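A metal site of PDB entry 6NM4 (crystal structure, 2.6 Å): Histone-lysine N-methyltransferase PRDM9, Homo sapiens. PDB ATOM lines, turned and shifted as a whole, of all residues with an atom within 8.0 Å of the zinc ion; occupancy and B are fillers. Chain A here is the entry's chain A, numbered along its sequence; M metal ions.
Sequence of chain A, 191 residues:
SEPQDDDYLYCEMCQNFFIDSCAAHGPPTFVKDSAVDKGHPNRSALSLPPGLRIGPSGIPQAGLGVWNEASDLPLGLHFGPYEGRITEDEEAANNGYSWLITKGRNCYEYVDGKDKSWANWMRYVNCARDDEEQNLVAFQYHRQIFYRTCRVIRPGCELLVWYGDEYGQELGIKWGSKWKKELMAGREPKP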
ATOM      1  N   TYR A  10     -14.651  27.828   9.229  1.00  0.00           N
ATOM      2  CA  TYR A  10     -13.662  27.722  10.297  1.00  0.00           C
ATOM      3  C   TYR A  10     -13.861  28.830  11.275  1.00  0.00           C
ATOM      4  O   TYR A  10     -13.931  29.960  10.882  1.00  0.00           O
ATOM      5  CB  TYR A  10     -12.273  27.808   9.693  1.00  0.00           C
ATOM      6  CG  TYR A  10     -11.147  27.651  10.695  1.00  0.00           C
ATOM      7  CD1 TYR A  10     -10.675  26.392  11.085  1.00  0.00           C
ATOM      8  CD2 TYR A  10     -10.545  28.765  11.239  1.00  0.00           C
ATOM      9  CE1 TYR A  10      -9.628  26.289  11.990  1.00  0.00           C
ATOM     10  CE2 TYR A  10      -9.505  28.652  12.155  1.00  0.00           C
ATOM     11  CZ  TYR A  10      -9.053  27.416  12.511  1.00  0.00           C
ATOM     12  OH  TYR A  10      -8.030  27.327  13.403  1.00  0.00           O
ATOM     13  N   CYS A  11     -13.959  28.482  12.560  1.00  0.00           N
ATOM     14  CA  CYS A  11     -14.175  29.484  13.594  1.00  0.00           C
ATOM     15  C   CYS A  11     -12.860  29.946  14.164  1.00  0.00           C
ATOM     16  O   CYS A  11     -12.171  29.180  14.842  1.00  0.00           O
ATOM     17  CB  CYS A  11     -15.028  28.947  14.725  1.00  0.00           C
ATOM     18  SG  CYS A  11     -15.348  30.269  15.920  1.00  0.00           S
ATOM     19  N   GLU A  12     -12.518  31.202  13.930  1.00  0.00           N
ATOM     20  CA  GLU A  12     -11.182  31.645  14.282  1.00  0.00           C
ATOM     21  C   GLU A  12     -10.967  31.753  15.792  1.00  0.00           C
ATOM     22  O   GLU A  12      -9.837  31.604  16.228  1.00  0.00           O
ATOM     23  CB  GLU A  12     -10.818  32.911  13.541  1.00  0.00           C
ATOM     24  CG  GLU A  12      -9.322  33.007  13.275  1.00  0.00           C
ATOM     25  CD  GLU A  12      -8.845  32.488  11.919  1.00  0.00           C
ATOM     26  OE1 GLU A  12      -7.653  32.136  11.854  1.00  0.00           O
ATOM     27  OE2 GLU A  12      -9.600  32.496  10.910  1.00  0.00           O
ATOM     28  N   MET A  13     -12.040  31.926  16.576  1.00  0.00           N
ATOM     29  CA  MET A  13     -11.945  31.929  18.076  1.00  0.00           C
ATOM     30  C   MET A  13     -11.776  30.554  18.758  1.00  0.00           C
ATOM     31  O   MET A  13     -10.944  30.403  19.645  1.00  0.00           O
ATOM     32  CB  MET A  13     -13.181  32.620  18.694  1.00  0.00           C
ATOM     33  CG  MET A  13     -13.176  34.124  18.647  1.00  0.00           C
ATOM     34  SD  MET A  13     -14.730  34.720  17.974  1.00  0.00           S
ATOM     35  CE  MET A  13     -14.522  34.356  16.210  1.00  0.00           C
ATOM     36  N   CYS A  14     -12.600  29.585  18.378  1.00  0.00           N
ATOM     37  CA  CYS A  14     -12.423  28.189  18.763  1.00  0.00           C
ATOM     38  C   CYS A  14     -11.181  27.516  18.166  1.00  0.00           C
ATOM     39  O   CYS A  14     -10.681  26.541  18.707  1.00  0.00           O
ATOM     40  CB  CYS A  14     -13.589  27.353  18.233  1.00  0.00           C
ATOM     41  SG  CYS A  14     -15.198  27.710  18.949  1.00  0.00           S
ATOM     42  N   GLN A  15     -10.745  28.006  17.001  1.00  0.00           N
ATOM     43  CA  GLN A  15      -9.733  27.316  16.185  1.00  0.00           C
ATOM     44  C   GLN A  15     -10.184  25.913  15.753  1.00  0.00           C
ATOM     45  O   GLN A  15      -9.422  24.970  15.753  1.00  0.00           O
ATOM     46  CB  GLN A  15      -8.361  27.260  16.877  1.00  0.00           C
ATOM     47  CG  GLN A  15      -7.854  28.616  17.361  1.00  0.00           C
ATOM     48  CD  GLN A  15      -6.668  29.133  16.562  1.00  0.00           C
ATOM     49  OE1 GLN A  15      -5.512  28.861  16.914  1.00  0.00           O
ATOM     50  NE2 GLN A  15      -6.946  29.919  15.498  1.00  0.00           N
ATOM     51  N   ASN A  16     -11.446  25.779  15.384  1.00  0.00           N
ATOM     52  CA  ASN A  16     -11.871  24.547  14.745  1.00  0.00           C
ATOM     53  C   ASN A  16     -12.925  24.754  13.698  1.00  0.00           C
ATOM     54  O   ASN A  16     -13.534  25.809  13.605  1.00  0.00           O
ATOM     55  CB  ASN A  16     -12.313  23.476  15.782  1.00  0.00           C
ATOM     56  CG  ASN A  16     -13.060  24.057  16.950  1.00  0.00           C
ATOM     57  OD1 ASN A  16     -14.132  24.630  16.765  1.00  0.00           O
ATOM     58  ND2 ASN A  16     -12.511  23.908  18.157  1.00  0.00           N
ATOM     59  N   PHE A  17     -13.113  23.718  12.889  1.00  0.00           N
ATOM     60  CA  PHE A  17     -14.059  23.704  11.796  1.00  0.00           C
ATOM     61  C   PHE A  17     -15.470  23.449  12.302  1.00  0.00           C
ATOM     62  O   PHE A  17     -15.661  22.895  13.380  1.00  0.00           O
ATOM     63  CB  PHE A  17     -13.644  22.641  10.771  1.00  0.00           C
ATOM     64  CG  PHE A  17     -12.336  22.971  10.083  1.00  0.00           C
ATOM     65  CD1 PHE A  17     -12.311  23.749   8.953  1.00  0.00           C
ATOM     66  CD2 PHE A  17     -11.139  22.519  10.592  1.00  0.00           C
ATOM     67  CE1 PHE A  17     -11.110  24.087   8.328  1.00  0.00           C
ATOM     68  CE2 PHE A  17      -9.934  22.835   9.983  1.00  0.00           C
ATOM     69  CZ  PHE A  17      -9.920  23.625   8.847  1.00  0.00           C
ATOM     70  N   PHE A  18     -16.443  23.907  11.522  1.00  0.00           N
ATOM     71  CA  PHE A  18     -17.846  23.664  11.797  1.00  0.00           C
ATOM     72  C   PHE A  18     -18.617  23.614  10.483  1.00  0.00           C
ATOM     73  O   PHE A  18     -18.044  23.887   9.411  1.00  0.00           O
ATOM     74  CB  PHE A  18     -18.417  24.722  12.750  1.00  0.00           C
ATOM     75  CG  PHE A  18     -18.466  26.119  12.193  1.00  0.00           C
ATOM     76  CD1 PHE A  18     -17.380  26.999  12.333  1.00  0.00           C
ATOM     77  CD2 PHE A  18     -19.629  26.599  11.585  1.00  0.00           C
ATOM     78  CE1 PHE A  18     -17.438  28.281  11.828  1.00  0.00           C
ATOM     79  CE2 PHE A  18     -19.696  27.901  11.085  1.00  0.00           C
ATOM     80  CZ  PHE A  18     -18.602  28.741  11.217  1.00  0.00           C
ATOM     81  N   SER A  21     -23.038  26.642  11.886  1.00  0.00           N
ATOM     82  CA  SER A  21     -22.734  27.588  12.923  1.00  0.00           C
ATOM     83  C   SER A  21     -21.825  26.966  13.964  1.00  0.00           C
ATOM     84  O   SER A  21     -21.898  25.765  14.222  1.00  0.00           O
ATOM     85  CB  SER A  21     -24.031  28.106  13.591  1.00  0.00           C
ATOM     86  OG  SER A  21     -23.899  28.259  14.993  1.00  0.00           O
ATOM     87  N   CYS A  22     -20.950  27.782  14.532  1.00  0.00           N
ATOM     88  CA  CYS A  22     -20.179  27.415  15.693  1.00  0.00           C
ATOM     89  C   CYS A  22     -21.118  27.490  16.878  1.00  0.00           C
ATOM     90  O   CYS A  22     -21.853  28.495  17.045  1.00  0.00           O
ATOM     91  CB  CYS A  22     -19.000  28.364  15.898  1.00  0.00           C
ATOM     92  SG  CYS A  22     -18.024  27.888  17.344  1.00  0.00           S
ATOM     93  N   ALA A  23     -21.103  26.450  17.694  1.00  0.00           N
ATOM     94  CA  ALA A  23     -22.006  26.347  18.838  1.00  0.00           C
ATOM     95  C   ALA A  23     -21.754  27.438  19.865  1.00  0.00           C
ATOM     96  O   ALA A  23     -22.636  27.762  20.654  1.00  0.00           O
ATOM     97  CB  ALA A  23     -21.921  24.969  19.481  1.00  0.00           C
ATOM     98  N   ALA A  24     -20.563  28.027  19.846  1.00  0.00           N
ATOM     99  CA  ALA A  24     -20.244  29.124  20.782  1.00  0.00           C
ATOM    100  C   ALA A  24     -20.255  30.508  20.140  1.00  0.00           C
ATOM    101  O   ALA A  24     -20.481  31.483  20.850  1.00  0.00           O
ATOM    102  CB  ALA A  24     -18.909  28.865  21.503  1.00  0.00           C
ATOM    103  N   HIS A  25     -19.988  30.637  18.845  1.00  0.00           N
ATOM    104  CA  HIS A  25     -19.828  31.981  18.223  1.00  0.00           C
ATOM    105  C   HIS A  25     -20.675  32.238  16.987  1.00  0.00           C
ATOM    106  O   HIS A  25     -20.553  33.282  16.361  1.00  0.00           O
ATOM    107  CB  HIS A  25     -18.359  32.226  17.887  1.00  0.00           C
ATOM    108  CG  HIS A  25     -17.429  32.024  19.044  1.00  0.00           C
ATOM    109  ND1 HIS A  25     -16.678  30.875  19.201  1.00  0.00           N
ATOM    110  CD2 HIS A  25     -17.151  32.807  20.112  1.00  0.00           C
ATOM    111  CE1 HIS A  25     -15.990  30.958  20.333  1.00  0.00           C
ATOM    112  NE2 HIS A  25     -16.261  32.120  20.910  1.00  0.00           N
ATOM    113  N   GLY A  26     -21.543  31.299  16.632  1.00  0.00           N
ATOM    114  CA  GLY A  26     -22.596  31.529  15.661  1.00  0.00           C
ATOM    115  C   GLY A  26     -22.188  31.324  14.225  1.00  0.00           C
ATOM    116  O   GLY A  26     -21.045  30.989  13.915  1.00  0.00           O
HETATM  117 ZN    ZN M   1     -16.300  29.381  17.781  1.00  0.00          ZN
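The side-chain sulfur (SG) of Cys 11 lies close to the backbone NH (N) of Met 13.
The backbone carbonyl oxygen (O) of Cys 14 sits at hydrogen-bond distance from the side-chain amide nitrogen (ND2) of Asn 16.
N of Cys 11 lies within hydrogen-bond range of O of Asn 16, at 2.9 Å.
The backbone NH (N) of Ala 24 lies close to the side-chain sulfur (SG) of Cys 22.
Four residues have an atom within 4 Å of the zinc ion: Cys 11, Cys 14, Cys 22 and His 25.
The nearest printed residue that does not touch the zinc ion is Ala 24 (4.6 Å).
A ring nitrogen (ND1) of His 25 is bound to the zinc ion.
SG of Cys 11 is bound to the zinc ion (2.3 Å).
SG of Cys 14 binds the zinc ion, 2.3 Å away.
The side-chain sulfur (SG) of Cys 22 binds the zinc ion, 2.3 Å away.
The zinc ion has four donor atoms within binding distance.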
